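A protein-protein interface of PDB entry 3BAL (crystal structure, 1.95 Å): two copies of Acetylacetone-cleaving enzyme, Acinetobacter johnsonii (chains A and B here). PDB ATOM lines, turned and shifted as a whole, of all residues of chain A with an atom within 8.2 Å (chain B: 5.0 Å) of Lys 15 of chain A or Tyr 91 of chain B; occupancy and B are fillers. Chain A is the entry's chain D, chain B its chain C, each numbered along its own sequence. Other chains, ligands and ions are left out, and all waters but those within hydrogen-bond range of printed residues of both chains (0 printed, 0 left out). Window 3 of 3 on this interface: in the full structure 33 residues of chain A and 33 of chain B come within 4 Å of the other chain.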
ATOM      1  N   GLU A  12      -1.429 -17.172 -18.086  1.00  0.00           N
ATOM      2  CA  GLU A  12      -2.543 -17.093 -17.137  1.00  0.00           C
ATOM      3  C   GLU A  12      -3.751 -17.912 -17.558  1.00  0.00           C
ATOM      4  O   GLU A  12      -4.020 -18.071 -18.749  1.00  0.00           O
ATOM      5  CB  GLU A  12      -3.014 -15.646 -16.977  1.00  0.00           C
ATOM      6  CG  GLU A  12      -2.056 -14.726 -16.253  1.00  0.00           C
ATOM      7  CD  GLU A  12      -2.395 -13.260 -16.471  1.00  0.00           C
ATOM      8  OE1 GLU A  12      -3.587 -12.932 -16.679  1.00  0.00           O
ATOM      9  OE2 GLU A  12      -1.468 -12.427 -16.421  1.00  0.00           O
ATOM     10  N   TYR A  13      -4.475 -18.428 -16.566  1.00  0.00           N
ATOM     11  CA  TYR A  13      -5.692 -19.193 -16.804  1.00  0.00           C
ATOM     12  C   TYR A  13      -6.729 -18.680 -15.813  1.00  0.00           C
ATOM     13  O   TYR A  13      -6.457 -18.587 -14.620  1.00  0.00           O
ATOM     14  CB  TYR A  13      -5.469 -20.696 -16.592  1.00  0.00           C
ATOM     15  CG  TYR A  13      -6.771 -21.472 -16.529  1.00  0.00           C
ATOM     16  CD1 TYR A  13      -7.624 -21.540 -17.632  1.00  0.00           C
ATOM     17  CD2 TYR A  13      -7.178 -22.086 -15.347  1.00  0.00           C
ATOM     18  CE1 TYR A  13      -8.847 -22.196 -17.554  1.00  0.00           C
ATOM     19  CE2 TYR A  13      -8.401 -22.744 -15.258  1.00  0.00           C
ATOM     20  CZ  TYR A  13      -9.229 -22.799 -16.362  1.00  0.00           C
ATOM     21  OH  TYR A  13     -10.432 -23.468 -16.280  1.00  0.00           O
ATOM     22  N   VAL A  14      -7.908 -18.323 -16.310  1.00  0.00           N
ATOM     23  CA  VAL A  14      -8.967 -17.812 -15.446  1.00  0.00           C
ATOM     24  C   VAL A  14     -10.277 -18.540 -15.735  1.00  0.00           C
ATOM     25  O   VAL A  14     -10.769 -18.525 -16.869  1.00  0.00           O
ATOM     26  CB  VAL A  14      -9.197 -16.284 -15.658  1.00  0.00           C
ATOM     27  CG1 VAL A  14     -10.337 -15.795 -14.773  1.00  0.00           C
ATOM     28  CG2 VAL A  14      -7.925 -15.508 -15.353  1.00  0.00           C
ATOM     29  N   LYS A  15     -10.834 -19.192 -14.721  1.00  0.00           N
ATOM     30  CA  LYS A  15     -12.099 -19.891 -14.907  1.00  0.00           C
ATOM     31  C   LYS A  15     -13.216 -18.871 -14.772  1.00  0.00           C
ATOM     32  O   LYS A  15     -13.271 -18.129 -13.794  1.00  0.00           O
ATOM     33  CB  LYS A  15     -12.296 -20.986 -13.856  1.00  0.00           C
ATOM     34  CG  LYS A  15     -13.632 -21.729 -13.993  1.00  0.00           C
ATOM     35  CD  LYS A  15     -13.696 -22.528 -15.291  1.00  0.00           C
ATOM     36  CE  LYS A  15     -14.991 -23.317 -15.409  1.00  0.00           C
ATOM     37  NZ  LYS A  15     -16.204 -22.447 -15.429  1.00  0.00           N
ATOM     38  N   ILE A  16     -14.102 -18.839 -15.757  1.00  0.00           N
ATOM     39  CA  ILE A  16     -15.214 -17.904 -15.738  1.00  0.00           C
ATOM     40  C   ILE A  16     -16.405 -18.545 -15.037  1.00  0.00           C
ATOM     41  O   ILE A  16     -17.134 -19.348 -15.623  1.00  0.00           O
ATOM     42  CB  ILE A  16     -15.608 -17.483 -17.168  1.00  0.00           C
ATOM     43  CG1 ILE A  16     -14.409 -16.800 -17.847  1.00  0.00           C
ATOM     44  CG2 ILE A  16     -16.807 -16.543 -17.121  1.00  0.00           C
ATOM     45  CD1 ILE A  16     -14.633 -16.450 -19.309  1.00  0.00           C
ATOM     46  N   SER A  17     -16.587 -18.179 -13.771  1.00  0.00           N
ATOM     47  CA  SER A  17     -17.665 -18.705 -12.945  1.00  0.00           C
ATOM     48  C   SER A  17     -18.705 -17.621 -12.683  1.00  0.00           C
ATOM     49  O   SER A  17     -18.374 -16.435 -12.610  1.00  0.00           O
ATOM     50  CB  SER A  17     -17.082 -19.205 -11.614  1.00  0.00           C
ATOM     51  OG  SER A  17     -18.101 -19.601 -10.709  1.00  0.00           O
ATOM     52  N   ASP A  18     -19.965 -18.020 -12.545  1.00  0.00           N
ATOM     53  CA  ASP A  18     -21.012 -17.047 -12.273  1.00  0.00           C
ATOM     54  C   ASP A  18     -20.815 -16.415 -10.902  1.00  0.00           C
ATOM     55  O   ASP A  18     -21.387 -15.372 -10.610  1.00  0.00           O
ATOM     56  CB  ASP A  18     -22.387 -17.706 -12.360  1.00  0.00           C
ATOM     57  CG  ASP A  18     -22.684 -18.225 -13.745  1.00  0.00           C
ATOM     58  OD1 ASP A  18     -22.388 -17.504 -14.717  1.00  0.00           O
ATOM     59  OD2 ASP A  18     -23.210 -19.351 -13.869  1.00  0.00           O
ATOM     60  N   ASN A  19     -19.994 -17.044 -10.063  1.00  0.00           N
ATOM     61  CA  ASN A  19     -19.727 -16.518  -8.717  1.00  0.00           C
ATOM     62  C   ASN A  19     -19.023 -15.182  -8.774  1.00  0.00           C
ATOM     63  O   ASN A  19     -19.102 -14.386  -7.837  1.00  0.00           O
ATOM     64  CB  ASN A  19     -18.800 -17.431  -7.912  1.00  0.00           C
ATOM     65  CG  ASN A  19     -19.434 -18.739  -7.556  1.00  0.00           C
ATOM     66  OD1 ASN A  19     -19.104 -19.778  -8.130  1.00  0.00           O
ATOM     67  ND2 ASN A  19     -20.355 -18.705  -6.599  1.00  0.00           N
ATOM     68  N   ASN A  20     -18.324 -14.943  -9.876  1.00  0.00           N
ATOM     69  CA  ASN A  20     -17.541 -13.731 -10.006  1.00  0.00           C
ATOM     70  C   ASN A  20     -18.180 -12.518 -10.671  1.00  0.00           C
ATOM     71  O   ASN A  20     -17.594 -11.435 -10.649  1.00  0.00           O
ATOM     72  CB  ASN A  20     -16.216 -14.085 -10.691  1.00  0.00           C
ATOM     73  CG  ASN A  20     -15.475 -15.220  -9.978  1.00  0.00           C
ATOM     74  OD1 ASN A  20     -16.060 -16.265  -9.677  1.00  0.00           O
ATOM     75  ND2 ASN A  20     -14.184 -15.022  -9.718  1.00  0.00           N
ATOM     76  N   TYR A  21     -19.366 -12.669 -11.256  1.00  0.00           N
ATOM     77  CA  TYR A  21     -20.003 -11.513 -11.891  1.00  0.00           C
ATOM     78  C   TYR A  21     -20.539 -10.547 -10.845  1.00  0.00           C
ATOM     79  O   TYR A  21     -21.286 -10.945  -9.958  1.00  0.00           O
ATOM     80  CB  TYR A  21     -21.161 -11.928 -12.800  1.00  0.00           C
ATOM     81  CG  TYR A  21     -20.744 -12.510 -14.131  1.00  0.00           C
ATOM     82  CD1 TYR A  21     -20.605 -13.890 -14.301  1.00  0.00           C
ATOM     83  CD2 TYR A  21     -20.509 -11.682 -15.226  1.00  0.00           C
ATOM     84  CE1 TYR A  21     -20.249 -14.432 -15.535  1.00  0.00           C
ATOM     85  CE2 TYR A  21     -20.152 -12.209 -16.463  1.00  0.00           C
ATOM     86  CZ  TYR A  21     -20.024 -13.587 -16.612  1.00  0.00           C
ATOM     87  OH  TYR A  21     -19.679 -14.118 -17.836  1.00  0.00           O
ATOM     88  N   GLN A  36     -17.130  -9.154 -15.318  1.00  0.00           N
ATOM     89  CA  GLN A  36     -15.950  -9.798 -14.740  1.00  0.00           C
ATOM     90  C   GLN A  36     -14.710  -9.289 -15.469  1.00  0.00           C
ATOM     91  O   GLN A  36     -14.665  -9.303 -16.692  1.00  0.00           O
ATOM     92  CB  GLN A  36     -15.986 -11.318 -14.930  1.00  0.00           C
ATOM     93  CG  GLN A  36     -16.847 -12.089 -13.969  1.00  0.00           C
ATOM     94  CD  GLN A  36     -16.520 -13.576 -13.985  1.00  0.00           C
ATOM     95  OE1 GLN A  36     -15.354 -13.968 -13.845  1.00  0.00           O
ATOM     96  NE2 GLN A  36     -17.542 -14.407 -14.145  1.00  0.00           N
ATOM     97  N   LEU A  37     -13.710  -8.838 -14.723  1.00  0.00           N
ATOM     98  CA  LEU A  37     -12.470  -8.407 -15.342  1.00  0.00           C
ATOM     99  C   LEU A  37     -11.674  -9.713 -15.468  1.00  0.00           C
ATOM    100  O   LEU A  37     -11.622 -10.499 -14.517  1.00  0.00           O
ATOM    101  CB  LEU A  37     -11.739  -7.407 -14.443  1.00  0.00           C
ATOM    102  CG  LEU A  37     -10.414  -6.864 -14.978  1.00  0.00           C
ATOM    103  CD1 LEU A  37     -10.630  -6.175 -16.316  1.00  0.00           C
ATOM    104  CD2 LEU A  37      -9.817  -5.910 -13.959  1.00  0.00           C
ATOM    105  N   LEU A  38     -11.077  -9.955 -16.635  1.00  0.00           N
ATOM    106  CA  LEU A  38     -10.321 -11.186 -16.873  1.00  0.00           C
ATOM    107  C   LEU A  38      -8.803 -11.025 -16.936  1.00  0.00           C
ATOM    108  O   LEU A  38      -8.067 -11.904 -16.480  1.00  0.00           O
ATOM    109  CB  LEU A  38     -10.803 -11.847 -18.172  1.00  0.00           C
ATOM    110  CG  LEU A  38     -12.259 -12.316 -18.208  1.00  0.00           C
ATOM    111  CD1 LEU A  38     -12.658 -12.684 -19.634  1.00  0.00           C
ATOM    112  CD2 LEU A  38     -12.434 -13.503 -17.271  1.00  0.00           C
ATOM    113  N   LEU B  72     -12.344 -20.089 -24.233  1.00  0.00           N
ATOM    114  CA  LEU B  72     -12.868 -21.445 -24.431  1.00  0.00           C
ATOM    115  C   LEU B  72     -14.354 -21.414 -24.092  1.00  0.00           C
ATOM    116  O   LEU B  72     -14.738 -21.321 -22.927  1.00  0.00           O
ATOM    117  CB  LEU B  72     -12.153 -22.445 -23.510  1.00  0.00           C
ATOM    118  CG  LEU B  72     -12.526 -23.936 -23.628  1.00  0.00           C
ATOM    119  CD1 LEU B  72     -12.147 -24.461 -25.017  1.00  0.00           C
ATOM    120  CD2 LEU B  72     -11.812 -24.737 -22.543  1.00  0.00           C
ATOM    121  N   GLY B  75     -16.262 -27.238 -24.120  1.00  0.00           N
ATOM    122  CA  GLY B  75     -15.280 -28.301 -23.993  1.00  0.00           C
ATOM    123  C   GLY B  75     -14.172 -28.157 -22.968  1.00  0.00           C
ATOM    124  O   GLY B  75     -14.329 -27.510 -21.931  1.00  0.00           O
ATOM    125  N   LYS B  76     -13.042 -28.788 -23.274  1.00  0.00           N
ATOM    126  CA  LYS B  76     -11.880 -28.790 -22.397  1.00  0.00           C
ATOM    127  C   LYS B  76     -10.618 -28.766 -23.239  1.00  0.00           C
ATOM    128  O   LYS B  76     -10.536 -29.433 -24.266  1.00  0.00           O
ATOM    129  CB  LYS B  76     -11.890 -30.043 -21.506  1.00  0.00           C
ATOM    130  CG  LYS B  76     -10.675 -30.138 -20.598  1.00  0.00           C
ATOM    131  CD  LYS B  76     -10.931 -30.973 -19.357  1.00  0.00           C
ATOM    132  CE  LYS B  76     -10.685 -32.440 -19.577  1.00  0.00           C
ATOM    133  NZ  LYS B  76     -10.459 -33.136 -18.266  1.00  0.00           N
ATOM    134  N   THR B  89      -5.150 -26.695 -17.584  1.00  0.00           N
ATOM    135  CA  THR B  89      -6.256 -27.471 -18.118  1.00  0.00           C
ATOM    136  C   THR B  89      -7.466 -26.537 -18.023  1.00  0.00           C
ATOM    137  O   THR B  89      -7.887 -26.159 -16.928  1.00  0.00           O
ATOM    138  CB  THR B  89      -6.491 -28.762 -17.304  1.00  0.00           C
ATOM    139  OG1 THR B  89      -5.364 -29.635 -17.471  1.00  0.00           O
ATOM    140  CG2 THR B  89      -7.755 -29.472 -17.768  1.00  0.00           C
ATOM    141  N   ALA B  90      -8.001 -26.150 -19.177  1.00  0.00           N
ATOM    142  CA  ALA B  90      -9.133 -25.231 -19.237  1.00  0.00           C
ATOM    143  C   ALA B  90     -10.487 -25.919 -19.407  1.00  0.00           C
ATOM    144  O   ALA B  90     -10.612 -26.863 -20.185  1.00  0.00           O
ATOM    145  CB  ALA B  90      -8.919 -24.236 -20.376  1.00  0.00           C
ATOM    146  N   TYR B  91     -11.488 -25.439 -18.668  1.00  0.00           N
ATOM    147  CA  TYR B  91     -12.847 -25.968 -18.751  1.00  0.00           C
ATOM    148  C   TYR B  91     -13.757 -24.816 -19.173  1.00  0.00           C
ATOM    149  O   TYR B  91     -13.650 -23.710 -18.638  1.00  0.00           O
ATOM    150  CB  TYR B  91     -13.334 -26.501 -17.399  1.00  0.00           C
ATOM    151  CG  TYR B  91     -12.588 -27.709 -16.875  1.00  0.00           C
ATOM    152  CD1 TYR B  91     -11.396 -27.566 -16.157  1.00  0.00           C
ATOM    153  CD2 TYR B  91     -13.087 -28.997 -17.075  1.00  0.00           C
ATOM    154  CE1 TYR B  91     -10.725 -28.679 -15.650  1.00  0.00           C
ATOM    155  CE2 TYR B  91     -12.425 -30.115 -16.576  1.00  0.00           C
ATOM    156  CZ  TYR B  91     -11.247 -29.951 -15.864  1.00  0.00           C
ATOM    157  OH  TYR B  91     -10.594 -31.061 -15.377  1.00  0.00           O
ATOM    158  N   ALA B  92     -14.657 -25.065 -20.116  1.00  0.00           N
ATOM    159  CA  ALA B  92     -15.553 -24.013 -20.585  1.00  0.00           C
ATOM    160  C   ALA B  92     -16.651 -23.643 -19.579  1.00  0.00           C
ATOM    161  O   ALA B  92     -17.246 -24.514 -18.944  1.00  0.00           O
ATOM    162  CB  ALA B  92     -16.180 -24.422 -21.915  1.00  0.00           C
ATOM    163  N   PRO B  93     -16.921 -22.337 -19.410  1.00  0.00           N
ATOM    164  CA  PRO B  93     -16.245 -21.235 -20.109  1.00  0.00           C
ATOM    165  C   PRO B  93     -15.004 -20.784 -19.341  1.00  0.00           C
ATOM    166  O   PRO B  93     -15.000 -20.785 -18.112  1.00  0.00           O
ATOM    167  CB  PRO B  93     -17.316 -20.152 -20.146  1.00  0.00           C
ATOM    168  CG  PRO B  93     -18.003 -20.345 -18.829  1.00  0.00           C
ATOM    169  CD  PRO B  93     -18.133 -21.855 -18.721  1.00  0.00           C
ATOM    170  N   SER B  94     -13.946 -20.415 -20.054  1.00  0.00           N
ATOM    171  CA  SER B  94     -12.729 -19.949 -19.395  1.00  0.00           C
ATOM    172  C   SER B  94     -11.867 -19.089 -20.319  1.00  0.00           C
ATOM    173  O   SER B  94     -12.088 -19.034 -21.528  1.00  0.00           O
ATOM    174  CB  SER B  94     -11.911 -21.126 -18.831  1.00  0.00           C
ATOM    175  OG  SER B  94     -11.599 -22.089 -19.825  1.00  0.00           O
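The side-chain hydroxyl (OH) of Tyr 13 of chain A sits at hydrogen-bond distance from the backbone NH (N) of Tyr 91 of chain B, 3.3 Å away.
O of Pro 93 of chain B lies within hydrogen-bond range of NZ of Lys 15 of chain A.
The backbone carbonyl oxygen of Pro 93 of chain B lies within hydrogen-bond range of the backbone NH of Ile 16 of chain A (3.2 Å).
N of Leu 72 of chain B sits at hydrogen-bond distance from O of Ser 94 of chain B (2.9 Å).
The backbone carbonyl oxygen of Tyr 91 of chain B is in hydrogen-bond range of the side-chain hydroxyl of Ser 94 of chain B (2.9 Å).
No position is printed for both chains.
Of the 9 pairs that touch across the chains among the printed residues, none has its exchanged pair printed and touching as well.
Of the 9 printed residues of chain B, 5 touch a printed residue of chain A.
Printed residues of chain A that touch a printed residue of chain B: Tyr 13, Val 14, Lys 15 and Ile 16.
Hydrophobic or aromatic side chains of chain A within 4 Å of the printed part of chain B: Tyr 13 and Ile 16.
Among the printed residues, merely in contact across the chains: Tyr 13 of chain A with Thr 89 of chain B (3.7 Å), Tyr 13 of chain A with Ala 90 of chain B (3.5 Å), Tyr 13 of chain A with Ser 94 of chain B (3.5 Å), Val 14 of chain A with Ser 94 of chain B (3.5 Å), Lys 15 of chain A with Tyr 91 of chain B (3.5 Å) and Ile 16 of chain A with Ser 94 of chain B (3.9 Å).
Lys 15 of chain A touches just these residues of chain B: Tyr 91 and Pro 93.
Of chain A, only Tyr 13 (3.3 Å) and Lys 15 (3.5 Å) come within 4 Å of Tyr 91 of chain B.
No residue of chain A comes within 4 Å of Ala 92 of chain B.
Of the printed residues of chain A, Thr 89 of chain B touches Tyr 13 (3.7 Å).
Printed residues of chain B within 4 Å of Tyr 13 of chain A: Thr 89, Ala 90, Tyr 91 and Ser 94.
Lys 76 of chain B touches none of the printed residues of chain A.
The nearest residue of chain B that does not touch Lys 15 of chain A is Ser 94 of chain B (4.1 Å).
The nearest residue of chain A that does not touch Tyr 91 of chain B is Ile 16 of chain A (5.7 Å).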
